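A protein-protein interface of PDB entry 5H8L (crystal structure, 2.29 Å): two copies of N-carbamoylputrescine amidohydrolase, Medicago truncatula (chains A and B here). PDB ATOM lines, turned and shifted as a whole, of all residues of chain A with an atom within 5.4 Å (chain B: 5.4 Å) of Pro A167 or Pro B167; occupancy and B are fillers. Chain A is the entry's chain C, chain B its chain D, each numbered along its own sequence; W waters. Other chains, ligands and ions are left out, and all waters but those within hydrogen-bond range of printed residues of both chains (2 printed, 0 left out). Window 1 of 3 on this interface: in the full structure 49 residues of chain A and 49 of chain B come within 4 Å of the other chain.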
ATOM      1  N   TRP A 165     -19.865 -14.708  19.855  1.00  0.00           N
ATOM      2  CA  TRP A 165     -20.998 -15.096  20.677  1.00  0.00           C
ATOM      3  C   TRP A 165     -21.683 -13.869  21.367  1.00  0.00           C
ATOM      4  O   TRP A 165     -22.713 -14.006  22.101  1.00  0.00           O
ATOM      5  CB  TRP A 165     -20.550 -16.114  21.743  1.00  0.00           C
ATOM      6  CG  TRP A 165     -20.200 -17.487  21.171  1.00  0.00           C
ATOM      7  CD1 TRP A 165     -19.018 -17.866  20.663  1.00  0.00           C
ATOM      8  CD2 TRP A 165     -21.068 -18.636  21.096  1.00  0.00           C
ATOM      9  NE1 TRP A 165     -19.087 -19.180  20.212  1.00  0.00           N
ATOM     10  CE2 TRP A 165     -20.324 -19.686  20.515  1.00  0.00           C
ATOM     11  CE3 TRP A 165     -22.376 -18.891  21.514  1.00  0.00           C
ATOM     12  CZ2 TRP A 165     -20.857 -20.953  20.293  1.00  0.00           C
ATOM     13  CZ3 TRP A 165     -22.911 -20.136  21.251  1.00  0.00           C
ATOM     14  CH2 TRP A 165     -22.137 -21.169  20.643  1.00  0.00           C
ATOM     15  N   PHE A 166     -21.064 -12.707  21.171  1.00  0.00           N
ATOM     16  CA  PHE A 166     -21.396 -11.467  21.913  1.00  0.00           C
ATOM     17  C   PHE A 166     -22.126 -10.454  21.006  1.00  0.00           C
ATOM     18  O   PHE A 166     -21.551  -9.835  20.104  1.00  0.00           O
ATOM     19  CB  PHE A 166     -20.131 -10.860  22.506  1.00  0.00           C
ATOM     20  CG  PHE A 166     -19.507 -11.743  23.481  1.00  0.00           C
ATOM     21  CD1 PHE A 166     -18.640 -12.743  23.062  1.00  0.00           C
ATOM     22  CD2 PHE A 166     -19.856 -11.655  24.803  1.00  0.00           C
ATOM     23  CE1 PHE A 166     -18.122 -13.635  23.954  1.00  0.00           C
ATOM     24  CE2 PHE A 166     -19.327 -12.532  25.713  1.00  0.00           C
ATOM     25  CZ  PHE A 166     -18.468 -13.537  25.286  1.00  0.00           C
ATOM     26  N   PRO A 167     -23.398 -10.308  21.217  1.00  0.00           N
ATOM     27  CA  PRO A 167     -24.115  -9.339  20.357  1.00  0.00           C
ATOM     28  C   PRO A 167     -23.538  -7.947  20.425  1.00  0.00           C
ATOM     29  O   PRO A 167     -23.594  -7.238  19.435  1.00  0.00           O
ATOM     30  CB  PRO A 167     -25.551  -9.336  20.933  1.00  0.00           C
ATOM     31  CG  PRO A 167     -25.688 -10.681  21.557  1.00  0.00           C
ATOM     32  CD  PRO A 167     -24.303 -11.090  22.056  1.00  0.00           C
ATOM     33  N   GLU A 168     -22.954  -7.597  21.572  1.00  0.00           N
ATOM     34  CA  GLU A 168     -22.314  -6.257  21.781  1.00  0.00           C
ATOM     35  C   GLU A 168     -21.253  -5.958  20.736  1.00  0.00           C
ATOM     36  O   GLU A 168     -21.072  -4.804  20.298  1.00  0.00           O
ATOM     37  CB  GLU A 168     -21.731  -6.130  23.219  1.00  0.00           C
ATOM     38  CG  GLU A 168     -22.763  -6.198  24.327  1.00  0.00           C
ATOM     39  CD  GLU A 168     -23.025  -7.589  24.883  1.00  0.00           C
ATOM     40  OE1 GLU A 168     -22.847  -8.570  24.141  1.00  0.00           O
ATOM     41  OE2 GLU A 168     -23.443  -7.692  26.057  1.00  0.00           O
ATOM     42  N   ALA A 169     -20.553  -7.004  20.290  1.00  0.00           N
ATOM     43  CA  ALA A 169     -19.458  -6.760  19.349  1.00  0.00           C
ATOM     44  C   ALA A 169     -19.987  -6.466  17.970  1.00  0.00           C
ATOM     45  O   ALA A 169     -19.480  -5.595  17.258  1.00  0.00           O
ATOM     46  CB  ALA A 169     -18.503  -7.927  19.314  1.00  0.00           C
ATOM     47  N   ALA A 170     -20.937  -7.265  17.532  1.00  0.00           N
ATOM     48  CA  ALA A 170     -21.506  -7.046  16.234  1.00  0.00           C
ATOM     49  C   ALA A 170     -22.173  -5.650  16.194  1.00  0.00           C
ATOM     50  O   ALA A 170     -22.028  -4.917  15.246  1.00  0.00           O
ATOM     51  CB  ALA A 170     -22.504  -8.086  15.985  1.00  0.00           C
ATOM     52  N   ARG A 171     -22.885  -5.292  17.252  1.00  0.00           N
ATOM     53  CA  ARG A 171     -23.539  -3.998  17.280  1.00  0.00           C
ATOM     54  C   ARG A 171     -22.511  -2.876  17.279  1.00  0.00           C
ATOM     55  O   ARG A 171     -22.662  -1.873  16.572  1.00  0.00           O
ATOM     56  CB  ARG A 171     -24.433  -3.856  18.508  1.00  0.00           C
ATOM     57  CG  ARG A 171     -25.210  -2.548  18.535  1.00  0.00           C
ATOM     58  CD  ARG A 171     -26.336  -2.533  17.485  1.00  0.00           C
ATOM     59  NE  ARG A 171     -27.632  -2.833  18.093  1.00  0.00           N
ATOM     60  CZ  ARG A 171     -28.714  -3.186  17.407  1.00  0.00           C
ATOM     61  NH1 ARG A 171     -28.625  -3.438  16.140  1.00  0.00           N
ATOM     62  NH2 ARG A 171     -29.848  -3.398  18.031  1.00  0.00           N
ATOM     63  N   ALA A 172     -21.486  -3.014  18.096  1.00  0.00           N
ATOM     64  CA  ALA A 172     -20.439  -1.996  18.107  1.00  0.00           C
ATOM     65  C   ALA A 172     -19.832  -1.726  16.729  1.00  0.00           C
ATOM     66  O   ALA A 172     -19.571  -0.560  16.390  1.00  0.00           O
ATOM     67  CB  ALA A 172     -19.335  -2.373  19.099  1.00  0.00           C
ATOM     68  N   HIS A 209     -26.971 -12.031  14.863  1.00  0.00           N
ATOM     69  CA  HIS A 209     -26.248 -10.740  14.700  1.00  0.00           C
ATOM     70  C   HIS A 209     -26.493 -10.159  13.336  1.00  0.00           C
ATOM     71  O   HIS A 209     -26.637  -8.941  13.196  1.00  0.00           O
ATOM     72  CB  HIS A 209     -24.680 -10.862  14.811  1.00  0.00           C
ATOM     73  CG  HIS A 209     -24.189 -11.509  16.066  1.00  0.00           C
ATOM     74  ND1 HIS A 209     -24.836 -11.389  17.276  1.00  0.00           N
ATOM     75  CD2 HIS A 209     -23.138 -12.319  16.286  1.00  0.00           C
ATOM     76  CE1 HIS A 209     -24.213 -12.110  18.183  1.00  0.00           C
ATOM     77  NE2 HIS A 209     -23.160 -12.663  17.611  1.00  0.00           N
ATOM     78  N   ALA A 212     -30.126  -8.803  13.190  1.00  0.00           N
ATOM     79  CA  ALA A 212     -30.442  -7.677  14.122  1.00  0.00           C
ATOM     80  C   ALA A 212     -29.769  -6.384  13.706  1.00  0.00           C
ATOM     81  O   ALA A 212     -30.238  -5.274  14.074  1.00  0.00           O
ATOM     82  CB  ALA A 212     -29.974  -8.028  15.531  1.00  0.00           C
ATOM     83  N   ASN A 213     -28.639  -6.534  13.007  1.00  0.00           N
ATOM     84  CA  ASN A 213     -27.899  -5.421  12.451  1.00  0.00           C
ATOM     85  C   ASN A 213     -28.100  -5.201  10.956  1.00  0.00           C
ATOM     86  O   ASN A 213     -27.582  -4.233  10.417  1.00  0.00           O
ATOM     87  CB  ASN A 213     -26.417  -5.636  12.725  1.00  0.00           C
ATOM     88  CG  ASN A 213     -26.127  -5.536  14.188  1.00  0.00           C
ATOM     89  OD1 ASN A 213     -26.172  -4.442  14.756  1.00  0.00           O
ATOM     90  ND2 ASN A 213     -25.922  -6.694  14.849  1.00  0.00           N
ATOM     91  N   TRP B 165     -36.524  -7.095  18.506  1.00  0.00           N
ATOM     92  CA  TRP B 165     -35.504  -6.999  17.481  1.00  0.00           C
ATOM     93  C   TRP B 165     -34.161  -6.490  18.015  1.00  0.00           C
ATOM     94  O   TRP B 165     -33.159  -6.508  17.296  1.00  0.00           O
ATOM     95  CB  TRP B 165     -35.979  -6.066  16.366  1.00  0.00           C
ATOM     96  CG  TRP B 165     -37.149  -6.647  15.592  1.00  0.00           C
ATOM     97  CD1 TRP B 165     -38.473  -6.556  15.920  1.00  0.00           C
ATOM     98  CD2 TRP B 165     -37.082  -7.453  14.405  1.00  0.00           C
ATOM     99  NE1 TRP B 165     -39.226  -7.230  14.992  1.00  0.00           N
ATOM    100  CE2 TRP B 165     -38.402  -7.777  14.047  1.00  0.00           C
ATOM    101  CE3 TRP B 165     -36.034  -7.864  13.563  1.00  0.00           C
ATOM    102  CZ2 TRP B 165     -38.704  -8.545  12.932  1.00  0.00           C
ATOM    103  CZ3 TRP B 165     -36.336  -8.620  12.449  1.00  0.00           C
ATOM    104  CH2 TRP B 165     -37.668  -8.949  12.132  1.00  0.00           C
ATOM    105  N   PHE B 166     -34.154  -6.049  19.276  1.00  0.00           N
ATOM    106  CA  PHE B 166     -32.981  -5.401  19.910  1.00  0.00           C
ATOM    107  C   PHE B 166     -32.213  -6.261  20.926  1.00  0.00           C
ATOM    108  O   PHE B 166     -32.692  -6.473  22.033  1.00  0.00           O
ATOM    109  CB  PHE B 166     -33.433  -4.091  20.569  1.00  0.00           C
ATOM    110  CG  PHE B 166     -34.056  -3.136  19.581  1.00  0.00           C
ATOM    111  CD1 PHE B 166     -35.425  -3.270  19.215  1.00  0.00           C
ATOM    112  CD2 PHE B 166     -33.300  -2.192  18.960  1.00  0.00           C
ATOM    113  CE1 PHE B 166     -35.972  -2.463  18.246  1.00  0.00           C
ATOM    114  CE2 PHE B 166     -33.851  -1.398  17.998  1.00  0.00           C
ATOM    115  CZ  PHE B 166     -35.181  -1.543  17.619  1.00  0.00           C
ATOM    116  N   PRO B 167     -30.984  -6.707  20.565  1.00  0.00           N
ATOM    117  CA  PRO B 167     -30.212  -7.594  21.450  1.00  0.00           C
ATOM    118  C   PRO B 167     -29.991  -6.936  22.765  1.00  0.00           C
ATOM    119  O   PRO B 167     -29.923  -7.630  23.801  1.00  0.00           O
ATOM    120  CB  PRO B 167     -28.887  -7.762  20.711  1.00  0.00           C
ATOM    121  CG  PRO B 167     -29.271  -7.678  19.254  1.00  0.00           C
ATOM    122  CD  PRO B 167     -30.330  -6.559  19.248  1.00  0.00           C
ATOM    123  N   GLU B 168     -29.931  -5.607  22.745  1.00  0.00           N
ATOM    124  CA  GLU B 168     -29.717  -4.847  23.958  1.00  0.00           C
ATOM    125  C   GLU B 168     -30.771  -5.107  25.016  1.00  0.00           C
ATOM    126  O   GLU B 168     -30.477  -5.148  26.234  1.00  0.00           O
ATOM    127  CB  GLU B 168     -29.688  -3.333  23.660  1.00  0.00           C
ATOM    128  CG  GLU B 168     -28.476  -2.830  22.869  1.00  0.00           C
ATOM    129  CD  GLU B 168     -28.674  -2.742  21.361  1.00  0.00           C
ATOM    130  OE1 GLU B 168     -29.534  -3.468  20.817  1.00  0.00           O
ATOM    131  OE2 GLU B 168     -27.976  -1.934  20.725  1.00  0.00           O
ATOM    132  N   ALA B 169     -32.012  -5.272  24.592  1.00  0.00           N
ATOM    133  CA  ALA B 169     -33.072  -5.420  25.557  1.00  0.00           C
ATOM    134  C   ALA B 169     -32.979  -6.792  26.187  1.00  0.00           C
ATOM    135  O   ALA B 169     -33.165  -6.932  27.393  1.00  0.00           O
ATOM    136  CB  ALA B 169     -34.415  -5.252  24.899  1.00  0.00           C
ATOM    137  N   ALA B 170     -32.709  -7.799  25.364  1.00  0.00           N
ATOM    138  CA  ALA B 170     -32.562  -9.177  25.862  1.00  0.00           C
ATOM    139  C   ALA B 170     -31.367  -9.301  26.841  1.00  0.00           C
ATOM    140  O   ALA B 170     -31.471  -9.892  27.878  1.00  0.00           O
ATOM    141  CB  ALA B 170     -32.381 -10.127  24.701  1.00  0.00           C
ATOM    142  N   ARG B 171     -30.237  -8.710  26.492  1.00  0.00           N
ATOM    143  CA  ARG B 171     -29.053  -8.744  27.348  1.00  0.00           C
ATOM    144  C   ARG B 171     -29.345  -7.990  28.675  1.00  0.00           C
ATOM    145  O   ARG B 171     -28.981  -8.440  29.751  1.00  0.00           O
ATOM    146  CB  ARG B 171     -27.884  -8.099  26.605  1.00  0.00           C
ATOM    147  CG  ARG B 171     -26.571  -8.103  27.411  1.00  0.00           C
ATOM    148  CD  ARG B 171     -26.056  -9.525  27.527  1.00  0.00           C
ATOM    149  NE  ARG B 171     -24.986  -9.803  26.600  1.00  0.00           N
ATOM    150  CZ  ARG B 171     -24.600 -11.023  26.241  1.00  0.00           C
ATOM    151  NH1 ARG B 171     -25.335 -12.086  26.576  1.00  0.00           N
ATOM    152  NH2 ARG B 171     -23.567 -11.175  25.475  1.00  0.00           N
ATOM    153  N   ALA B 172     -30.076  -6.889  28.600  1.00  0.00           N
ATOM    154  CA  ALA B 172     -30.324  -6.078  29.796  1.00  0.00           C
ATOM    155  C   ALA B 172     -31.118  -6.846  30.810  1.00  0.00           C
ATOM    156  O   ALA B 172     -30.890  -6.740  32.028  1.00  0.00           O
ATOM    157  CB  ALA B 172     -31.062  -4.807  29.423  1.00  0.00           C
ATOM    158  N   HIS B 209     -31.096 -14.118  20.484  1.00  0.00           N
ATOM    159  CA  HIS B 209     -31.137 -13.658  21.862  1.00  0.00           C
ATOM    160  C   HIS B 209     -31.142 -14.829  22.814  1.00  0.00           C
ATOM    161  O   HIS B 209     -30.460 -14.818  23.862  1.00  0.00           O
ATOM    162  CB  HIS B 209     -32.455 -12.875  22.196  1.00  0.00           C
ATOM    163  CG  HIS B 209     -32.742 -11.683  21.312  1.00  0.00           C
ATOM    164  ND1 HIS B 209     -31.766 -10.998  20.623  1.00  0.00           N
ATOM    165  CD2 HIS B 209     -33.907 -11.065  21.011  1.00  0.00           C
ATOM    166  CE1 HIS B 209     -32.311 -10.002  19.945  1.00  0.00           C
ATOM    167  NE2 HIS B 209     -33.611 -10.031  20.150  1.00  0.00           N
ATOM    168  N   ALA B 212     -27.676 -16.346  22.840  1.00  0.00           N
ATOM    169  CA  ALA B 212     -26.586 -15.511  23.318  1.00  0.00           C
ATOM    170  C   ALA B 212     -26.651 -15.262  24.821  1.00  0.00           C
ATOM    171  O   ALA B 212     -25.656 -14.961  25.436  1.00  0.00           O
ATOM    172  CB  ALA B 212     -26.574 -14.211  22.584  1.00  0.00           C
ATOM    173  N   ASN B 213     -27.836 -15.379  25.391  1.00  0.00           N
ATOM    174  CA  ASN B 213     -28.021 -15.222  26.825  1.00  0.00           C
ATOM    175  C   ASN B 213     -28.267 -16.533  27.550  1.00  0.00           C
ATOM    176  O   ASN B 213     -28.292 -16.573  28.783  1.00  0.00           O
ATOM    177  CB  ASN B 213     -29.151 -14.252  27.078  1.00  0.00           C
ATOM    178  CG  ASN B 213     -28.817 -12.870  26.592  1.00  0.00           C
ATOM    179  OD1 ASN B 213     -28.067 -12.122  27.247  1.00  0.00           O
ATOM    180  ND2 ASN B 213     -29.360 -12.509  25.444  1.00  0.00           N
HETATM  181  O   HOH W   1     -23.223 -13.767  24.568  1.00  0.00           O
HETATM  182  O   HOH W   2     -31.606  -4.554  16.063  1.00  0.00           O
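Of the 11 printed residues of chain B, 6 touch a printed residue of chain A. Hydrophobic or aromatic side chains of chain B that line the printed part of chain A: Phe B166, Pro B167 and Ala B212. Of the 11 printed residues of chain A, 6 touch a printed residue of chain B. Along chain A the printed residues that touch a printed residue of chain B span positions 165 to 212.
Water W2 lies within hydrogen-bond range of O of Ala A212 (2.5 Å), O of Trp B165 (2.8 Å) and NH2 of Arg A171 (2.9 Å). Water W1 lies within hydrogen-bond range of the backbone carbonyl oxygen of Trp A165 (2.5 Å), the guanidinium group of Arg B171 (2.8 Å) and the backbone carbonyl oxygen of Ala B212 (2.8 Å).
Pro B167 touches just these residues of chain A: Pro A167 (3.7 Å), Arg A171 (3.4 Å) and Ala A212 (3.8 Å). Of the printed residues of chain B, Trp A165 touches Ala B212. Of the printed residues of chain A, Arg B171 touches Phe A166, Pro A167 and Glu A168. Of the printed residues of chain B, Glu A168 touches Arg B171. Of the printed residues of chain A, Phe B166 touches Arg A171 (3.8 Å). Printed residues of chain B within 4 Å of Ala A212: Trp B165 and Pro B167. The nearest printed residue of chain A that does not touch Pro B167 is Asn A213 (5.6 Å).
The guanidinium group (NH1) of Arg B171 sits at hydrogen-bond distance from the backbone carbonyl oxygen (O) of Ala B212. The guanidinium group (NH1) of Arg A171 sits at hydrogen-bond distance from the side-chain amide oxygen (OD1) of Asn A213 (3.0 Å). The guanidinium group (NH1) of Arg A171 is in hydrogen-bond range of the backbone carbonyl oxygen (O) of Ala A212 (3.2 Å). NH1 of Arg B171 sits at hydrogen-bond distance from OD1 of Asn B213, at 2.8 Å.
Trp A165 touches Ala B212, and with the chains exchanged Ala A212 touches Trp B165. Pro B167 touches its own counterpart, Pro A167. Pro A167 touches Arg B171, and with the chains exchanged Arg A171 touches Pro B167. Glu A168 touches Arg B171, and with the chains exchanged Arg A171 touches Glu B168. 11 positions are printed for both chains. Of the 11 pairs that touch across the chains among the printed residues, 11 have their exchanged pair printed and touching as well.
The side-chain carboxylate (OE2) of Glu B168 lies within salt-bridge range of the guanidinium group (NE) of Arg A171. OE2 of Glu A168 is in salt-bridge range of NE of Arg B171 (2.7 Å).
Among the printed residues, pairs that only touch across the chains: Arg A171 with Pro B167 (3.4 Å), Pro A167 with Arg B171 (3.5 Å), Pro A167 with Pro B167 (3.7 Å), Arg A171 with Phe B166 (3.8 Å), Pro A167 with Ala B212 (3.8 Å), Phe A166 with Arg B171 (3.8 Å), Ala A212 with Pro B167 (3.8 Å), Trp A165 with Ala B212 (3.9 Å) and Ala A212 with Trp B165 (3.9 Å).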
